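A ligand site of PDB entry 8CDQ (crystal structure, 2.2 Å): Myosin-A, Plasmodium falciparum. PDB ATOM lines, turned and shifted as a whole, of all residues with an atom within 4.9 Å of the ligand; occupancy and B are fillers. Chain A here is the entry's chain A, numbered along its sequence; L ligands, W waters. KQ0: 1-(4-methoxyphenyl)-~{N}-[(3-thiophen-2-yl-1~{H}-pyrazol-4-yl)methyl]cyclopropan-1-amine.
Water W1 bridges O of Ser 246 and N16 of the ligand.
Merely in contact with the ligand: Thr 489 (3.2 Å), Phe 485 (3.3 Å), Ser 246 (3.4 Å), Glu 482 (3.5 Å), Gly 249 (3.5 Å), Ile 470 (3.5 Å), Glu 273 (3.5 Å), Arg 247 (3.6 Å) and Ile 486 (3.9 Å).
Hydrophobic or aromatic side chains that line the ligand: Leu 271, Ile 470, Phe 471, Phe 485 and Ile 486.
The nearest printed residue that does not touch the ligand is Phe 270 (4.01 Å).
The side-chain amide nitrogen (ND2) of Asn 490 lies within hydrogen-bond range of the backbone carbonyl oxygen (O) of Phe 471.
O of Phe 485 lies within hydrogen-bond range of OG1 of Thr 489, 3.0 Å away.
N of Gly 249 sits at hydrogen-bond distance from O of Phe 270 (2.8 Å).
NH1 of Arg 247 lies within salt-bridge range of OE1 of Glu 273, 3.0 Å away.
The side-chain amide nitrogen of Asn 490 sits at hydrogen-bond distance from the backbone carbonyl oxygen of Ile 486 (2.9 Å).
O of Leu 271 is in hydrogen-bond range of N12 of the ligand, 2.8 Å away.
The backbone NH (N) of Phe 471 sits at hydrogen-bond distance from a nitrogen (N17) of the ligand (3.1 Å).
O of Phe 248 lies close to N16 of the ligand, at 3.4 Å.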
ATOM      1  N   SER A 246     -24.154 -22.135  -7.714  1.00  0.00           N
ATOM      2  CA  SER A 246     -23.859 -23.140  -8.744  1.00  0.00           C
ATOM      3  C   SER A 246     -23.404 -22.451 -10.028  1.00  0.00           C
ATOM      4  O   SER A 246     -24.178 -21.726 -10.645  1.00  0.00           O
ATOM      5  CB  SER A 246     -25.086 -23.992  -9.030  1.00  0.00           C
ATOM      6  OG  SER A 246     -25.591 -24.517  -7.821  1.00  0.00           O
ATOM      7  N   ARG A 247     -22.162 -22.705 -10.433  1.00  0.00           N
ATOM      8  CA  ARG A 247     -21.552 -22.073 -11.600  1.00  0.00           C
ATOM      9  C   ARG A 247     -21.574 -23.000 -12.796  1.00  0.00           C
ATOM     10  O   ARG A 247     -20.647 -23.008 -13.615  1.00  0.00           O
ATOM     11  CB  ARG A 247     -20.132 -21.651 -11.266  1.00  0.00           C
ATOM     12  CG  ARG A 247     -20.118 -20.846 -10.000  1.00  0.00           C
ATOM     13  CD  ARG A 247     -20.188 -19.419 -10.402  1.00  0.00           C
ATOM     14  NE  ARG A 247     -21.492 -18.833 -10.164  1.00  0.00           N
ATOM     15  CZ  ARG A 247     -21.853 -17.645 -10.615  1.00  0.00           C
ATOM     16  NH1 ARG A 247     -21.080 -16.946 -11.434  1.00  0.00           N
ATOM     17  NH2 ARG A 247     -23.027 -17.140 -10.221  1.00  0.00           N
ATOM     18  N   PHE A 248     -22.637 -23.776 -12.904  1.00  0.00           N
ATOM     19  CA  PHE A 248     -22.834 -24.701 -14.012  1.00  0.00           C
ATOM     20  C   PHE A 248     -24.314 -25.068 -14.010  1.00  0.00           C
ATOM     21  O   PHE A 248     -24.958 -25.002 -12.962  1.00  0.00           O
ATOM     22  CB  PHE A 248     -21.960 -25.947 -13.860  1.00  0.00           C
ATOM     23  CG  PHE A 248     -22.349 -26.822 -12.697  1.00  0.00           C
ATOM     24  CD1 PHE A 248     -21.984 -26.480 -11.411  1.00  0.00           C
ATOM     25  CD2 PHE A 248     -23.044 -28.005 -12.900  1.00  0.00           C
ATOM     26  CE1 PHE A 248     -22.338 -27.311 -10.340  1.00  0.00           C
ATOM     27  CE2 PHE A 248     -23.409 -28.819 -11.842  1.00  0.00           C
ATOM     28  CZ  PHE A 248     -23.056 -28.472 -10.562  1.00  0.00           C
ATOM     29  N   GLY A 249     -24.838 -25.419 -15.184  1.00  0.00           N
ATOM     30  CA  GLY A 249     -26.207 -25.918 -15.275  1.00  0.00           C
ATOM     31  C   GLY A 249     -26.170 -27.422 -15.085  1.00  0.00           C
ATOM     32  O   GLY A 249     -25.218 -28.082 -15.485  1.00  0.00           O
ATOM     33  N   PHE A 270     -23.397 -28.464 -17.613  1.00  0.00           N
ATOM     34  CA  PHE A 270     -22.984 -27.627 -18.740  1.00  0.00           C
ATOM     35  C   PHE A 270     -22.595 -26.215 -18.321  1.00  0.00           C
ATOM     36  O   PHE A 270     -23.022 -25.675 -17.291  1.00  0.00           O
ATOM     37  CB  PHE A 270     -24.033 -27.525 -19.839  1.00  0.00           C
ATOM     38  CG  PHE A 270     -25.412 -27.664 -19.367  1.00  0.00           C
ATOM     39  CD1 PHE A 270     -26.115 -26.570 -18.952  1.00  0.00           C
ATOM     40  CD2 PHE A 270     -26.023 -28.902 -19.371  1.00  0.00           C
ATOM     41  CE1 PHE A 270     -27.425 -26.703 -18.505  1.00  0.00           C
ATOM     42  CE2 PHE A 270     -27.301 -29.050 -18.948  1.00  0.00           C
ATOM     43  CZ  PHE A 270     -28.011 -27.969 -18.513  1.00  0.00           C
ATOM     44  N   LEU A 271     -21.757 -25.634 -19.184  1.00  0.00           N
ATOM     45  CA  LEU A 271     -21.293 -24.273 -19.092  1.00  0.00           C
ATOM     46  C   LEU A 271     -20.712 -23.971 -17.711  1.00  0.00           C
ATOM     47  O   LEU A 271     -21.142 -23.049 -16.998  1.00  0.00           O
ATOM     48  CB  LEU A 271     -22.419 -23.307 -19.446  1.00  0.00           C
ATOM     49  CG  LEU A 271     -22.698 -23.395 -20.952  1.00  0.00           C
ATOM     50  CD1 LEU A 271     -23.908 -22.536 -21.287  1.00  0.00           C
ATOM     51  CD2 LEU A 271     -21.467 -22.965 -21.757  1.00  0.00           C
ATOM     52  N   LEU A 272     -19.710 -24.775 -17.327  1.00  0.00           N
ATOM     53  CA  LEU A 272     -18.938 -24.456 -16.129  1.00  0.00           C
ATOM     54  C   LEU A 272     -18.247 -23.108 -16.325  1.00  0.00           C
ATOM     55  O   LEU A 272     -17.736 -22.791 -17.398  1.00  0.00           O
ATOM     56  CB  LEU A 272     -17.916 -25.563 -15.860  1.00  0.00           C
ATOM     57  CG  LEU A 272     -16.997 -25.326 -14.650  1.00  0.00           C
ATOM     58  CD1 LEU A 272     -17.756 -25.284 -13.310  1.00  0.00           C
ATOM     59  CD2 LEU A 272     -15.972 -26.393 -14.629  1.00  0.00           C
ATOM     60  N   GLU A 273     -18.256 -22.286 -15.275  1.00  0.00           N
ATOM     61  CA  GLU A 273     -17.665 -20.936 -15.348  1.00  0.00           C
ATOM     62  C   GLU A 273     -16.159 -21.054 -15.212  1.00  0.00           C
ATOM     63  O   GLU A 273     -15.576 -20.789 -14.157  1.00  0.00           O
ATOM     64  CB  GLU A 273     -18.225 -20.020 -14.270  1.00  0.00           C
ATOM     65  CG  GLU A 273     -17.888 -18.572 -14.497  1.00  0.00           C
ATOM     66  CD  GLU A 273     -18.463 -17.632 -13.450  1.00  0.00           C
ATOM     67  OE1 GLU A 273     -18.376 -17.938 -12.241  1.00  0.00           O
ATOM     68  OE2 GLU A 273     -19.008 -16.573 -13.842  1.00  0.00           O
ATOM     69  N   ASP A 469     -31.790 -27.780 -13.201  1.00  0.00           N
ATOM     70  CA  ASP A 469     -31.502 -26.779 -12.166  1.00  0.00           C
ATOM     71  C   ASP A 469     -30.696 -25.654 -12.832  1.00  0.00           C
ATOM     72  O   ASP A 469     -29.486 -25.819 -13.038  1.00  0.00           O
ATOM     73  CB  ASP A 469     -30.733 -27.425 -11.034  1.00  0.00           C
ATOM     74  CG  ASP A 469     -30.293 -26.456  -9.940  1.00  0.00           C
ATOM     75  OD1 ASP A 469     -30.134 -25.242 -10.209  1.00  0.00           O
ATOM     76  OD2 ASP A 469     -29.939 -26.922  -8.818  1.00  0.00           O
ATOM     77  N   ILE A 470     -31.322 -24.518 -13.169  1.00  0.00           N
ATOM     78  CA  ILE A 470     -30.653 -23.512 -14.002  1.00  0.00           C
ATOM     79  C   ILE A 470     -31.091 -22.090 -13.643  1.00  0.00           C
ATOM     80  O   ILE A 470     -32.163 -21.873 -13.087  1.00  0.00           O
ATOM     81  CB  ILE A 470     -30.941 -23.740 -15.497  1.00  0.00           C
ATOM     82  CG1 ILE A 470     -32.450 -23.797 -15.711  1.00  0.00           C
ATOM     83  CG2 ILE A 470     -30.249 -24.984 -16.034  1.00  0.00           C
ATOM     84  CD1 ILE A 470     -32.830 -23.559 -17.139  1.00  0.00           C
ATOM     85  N   PHE A 471     -30.254 -21.114 -14.008  1.00  0.00           N
ATOM     86  CA  PHE A 471     -30.702 -19.738 -13.975  1.00  0.00           C
ATOM     87  C   PHE A 471     -31.926 -19.579 -14.861  1.00  0.00           C
ATOM     88  O   PHE A 471     -32.057 -20.255 -15.882  1.00  0.00           O
ATOM     89  CB  PHE A 471     -29.585 -18.791 -14.453  1.00  0.00           C
ATOM     90  CG  PHE A 471     -28.492 -18.551 -13.437  1.00  0.00           C
ATOM     91  CD1 PHE A 471     -28.765 -18.042 -12.174  1.00  0.00           C
ATOM     92  CD2 PHE A 471     -27.149 -18.830 -13.745  1.00  0.00           C
ATOM     93  CE1 PHE A 471     -27.742 -17.816 -11.231  1.00  0.00           C
ATOM     94  CE2 PHE A 471     -26.117 -18.606 -12.805  1.00  0.00           C
ATOM     95  CZ  PHE A 471     -26.421 -18.102 -11.569  1.00  0.00           C
ATOM     96  N   GLU A 482     -22.222 -15.044 -21.482  1.00  0.00           N
ATOM     97  CA  GLU A 482     -22.787 -15.942 -20.478  1.00  0.00           C
ATOM     98  C   GLU A 482     -24.287 -15.761 -20.313  1.00  0.00           C
ATOM     99  O   GLU A 482     -25.035 -16.731 -20.174  1.00  0.00           O
ATOM    100  CB  GLU A 482     -22.084 -15.744 -19.140  1.00  0.00           C
ATOM    101  CG  GLU A 482     -20.633 -16.190 -19.130  1.00  0.00           C
ATOM    102  CD  GLU A 482     -19.659 -15.034 -19.178  1.00  0.00           C
ATOM    103  OE1 GLU A 482     -20.008 -13.944 -19.686  1.00  0.00           O
ATOM    104  OE2 GLU A 482     -18.521 -15.227 -18.694  1.00  0.00           O
ATOM    105  N   PHE A 485     -26.306 -17.108 -23.635  1.00  0.00           N
ATOM    106  CA  PHE A 485     -26.593 -18.538 -23.631  1.00  0.00           C
ATOM    107  C   PHE A 485     -27.701 -18.862 -22.627  1.00  0.00           C
ATOM    108  O   PHE A 485     -28.647 -19.607 -22.927  1.00  0.00           O
ATOM    109  CB  PHE A 485     -25.332 -19.342 -23.280  1.00  0.00           C
ATOM    110  CG  PHE A 485     -24.223 -19.220 -24.297  1.00  0.00           C
ATOM    111  CD1 PHE A 485     -24.489 -18.927 -25.616  1.00  0.00           C
ATOM    112  CD2 PHE A 485     -22.911 -19.455 -23.912  1.00  0.00           C
ATOM    113  CE1 PHE A 485     -23.463 -18.835 -26.535  1.00  0.00           C
ATOM    114  CE2 PHE A 485     -21.880 -19.369 -24.813  1.00  0.00           C
ATOM    115  CZ  PHE A 485     -22.155 -19.061 -26.136  1.00  0.00           C
ATOM    116  N   ILE A 486     -27.613 -18.305 -21.418  1.00  0.00           N
ATOM    117  CA  ILE A 486     -28.676 -18.511 -20.430  1.00  0.00           C
ATOM    118  C   ILE A 486     -30.026 -18.087 -21.002  1.00  0.00           C
ATOM    119  O   ILE A 486     -31.010 -18.822 -20.899  1.00  0.00           O
ATOM    120  CB  ILE A 486     -28.337 -17.754 -19.131  1.00  0.00           C
ATOM    121  CG1 ILE A 486     -27.083 -18.359 -18.485  1.00  0.00           C
ATOM    122  CG2 ILE A 486     -29.547 -17.765 -18.172  1.00  0.00           C
ATOM    123  CD1 ILE A 486     -26.624 -17.631 -17.226  1.00  0.00           C
ATOM    124  N   THR A 489     -31.353 -20.550 -23.543  1.00  0.00           N
ATOM    125  CA  THR A 489     -31.908 -21.710 -22.843  1.00  0.00           C
ATOM    126  C   THR A 489     -33.323 -21.444 -22.348  1.00  0.00           C
ATOM    127  O   THR A 489     -34.200 -22.314 -22.445  1.00  0.00           O
ATOM    128  CB  THR A 489     -31.043 -22.134 -21.641  1.00  0.00           C
ATOM    129  OG1 THR A 489     -29.681 -22.283 -22.020  1.00  0.00           O
ATOM    130  CG2 THR A 489     -31.524 -23.470 -21.114  1.00  0.00           C
ATOM    131  N   ASN A 490     -33.572 -20.261 -21.833  1.00  0.00           N
ATOM    132  CA  ASN A 490     -34.881 -19.998 -21.246  1.00  0.00           C
ATOM    133  C   ASN A 490     -35.933 -19.644 -22.273  1.00  0.00           C
ATOM    134  O   ASN A 490     -37.133 -19.830 -22.012  1.00  0.00           O
ATOM    135  CB  ASN A 490     -34.740 -18.897 -20.207  1.00  0.00           C
ATOM    136  CG  ASN A 490     -34.216 -19.441 -18.904  1.00  0.00           C
ATOM    137  OD1 ASN A 490     -34.982 -19.985 -18.112  1.00  0.00           O
ATOM    138  ND2 ASN A 490     -32.894 -19.345 -18.696  1.00  0.00           N
ATOM    139  N   ILE A 641     -17.284 -22.626 -27.636  1.00  0.00           N
ATOM    140  CA  ILE A 641     -18.253 -22.859 -26.572  1.00  0.00           C
ATOM    141  C   ILE A 641     -19.669 -22.786 -27.124  1.00  0.00           C
ATOM    142  O   ILE A 641     -20.493 -23.684 -26.876  1.00  0.00           O
ATOM    143  CB  ILE A 641     -18.048 -21.859 -25.430  1.00  0.00           C
ATOM    144  CG1 ILE A 641     -16.677 -22.070 -24.783  1.00  0.00           C
ATOM    145  CG2 ILE A 641     -19.130 -22.040 -24.386  1.00  0.00           C
ATOM    146  CD1 ILE A 641     -16.384 -21.148 -23.613  1.00  0.00           C
ATOM    147  N   PHE A 645     -22.213 -25.832 -27.128  1.00  0.00           N
ATOM    148  CA  PHE A 645     -23.351 -25.663 -26.247  1.00  0.00           C
ATOM    149  C   PHE A 645     -24.678 -25.809 -26.990  1.00  0.00           C
ATOM    150  O   PHE A 645     -25.620 -26.418 -26.489  1.00  0.00           O
ATOM    151  CB  PHE A 645     -23.328 -24.321 -25.510  1.00  0.00           C
ATOM    152  CG  PHE A 645     -24.524 -24.136 -24.620  1.00  0.00           C
ATOM    153  CD1 PHE A 645     -24.771 -25.057 -23.584  1.00  0.00           C
ATOM    154  CD2 PHE A 645     -25.447 -23.137 -24.841  1.00  0.00           C
ATOM    155  CE1 PHE A 645     -25.889 -24.961 -22.786  1.00  0.00           C
ATOM    156  CE2 PHE A 645     -26.575 -23.039 -24.040  1.00  0.00           C
ATOM    157  CZ  PHE A 645     -26.788 -23.948 -23.008  1.00  0.00           C
HETATM  158  C10 KQ0 L   1     -23.053 -19.020 -14.843  1.00  0.00           C
HETATM  159  N12 KQ0 L   1     -22.980 -21.311 -15.709  1.00  0.00           N
HETATM  160  C13 KQ0 L   1     -24.189 -21.836 -16.379  1.00  0.00           C
HETATM  161  C15 KQ0 L   1     -25.189 -21.952 -13.917  1.00  0.00           C
HETATM  162  C20 KQ0 L   1     -28.672 -21.727 -17.287  1.00  0.00           C
HETATM  163  C21 KQ0 L   1     -28.964 -21.937 -18.679  1.00  0.00           C
HETATM  164  C22 KQ0 L   1     -27.884 -22.471 -19.405  1.00  0.00           C
HETATM  165  C01 KQ0 L   1     -19.337 -19.282 -21.440  1.00  0.00           C
HETATM  166  C03 KQ0 L   1     -21.226 -19.491 -20.106  1.00  0.00           C
HETATM  167  C04 KQ0 L   1     -20.331 -19.815 -19.084  1.00  0.00           C
HETATM  168  C05 KQ0 L   1     -20.808 -19.953 -17.777  1.00  0.00           C
HETATM  169  C06 KQ0 L   1     -22.166 -19.781 -17.499  1.00  0.00           C
HETATM  170  C07 KQ0 L   1     -23.054 -19.468 -18.527  1.00  0.00           C
HETATM  171  C08 KQ0 L   1     -22.577 -19.330 -19.834  1.00  0.00           C
HETATM  172  C09 KQ0 L   1     -22.666 -19.905 -16.041  1.00  0.00           C
HETATM  173  C11 KQ0 L   1     -21.591 -19.330 -15.094  1.00  0.00           C
HETATM  174  C14 KQ0 L   1     -25.320 -21.961 -15.326  1.00  0.00           C
HETATM  175  C18 KQ0 L   1     -26.719 -22.038 -15.553  1.00  0.00           C
HETATM  176  C19 KQ0 L   1     -27.375 -22.081 -16.927  1.00  0.00           C
HETATM  177  N16 KQ0 L   1     -26.431 -22.028 -13.436  1.00  0.00           N
HETATM  178  N17 KQ0 L   1     -27.354 -22.089 -14.394  1.00  0.00           N
HETATM  179  O02 KQ0 L   1     -20.744 -19.362 -21.428  1.00  0.00           O
HETATM  180  S23 KQ0 L   1     -26.605 -22.644 -18.311  1.00  0.00           S
HETATM  181  O   HOH W   1     -26.967 -21.741 -10.677  1.00  0.00           O
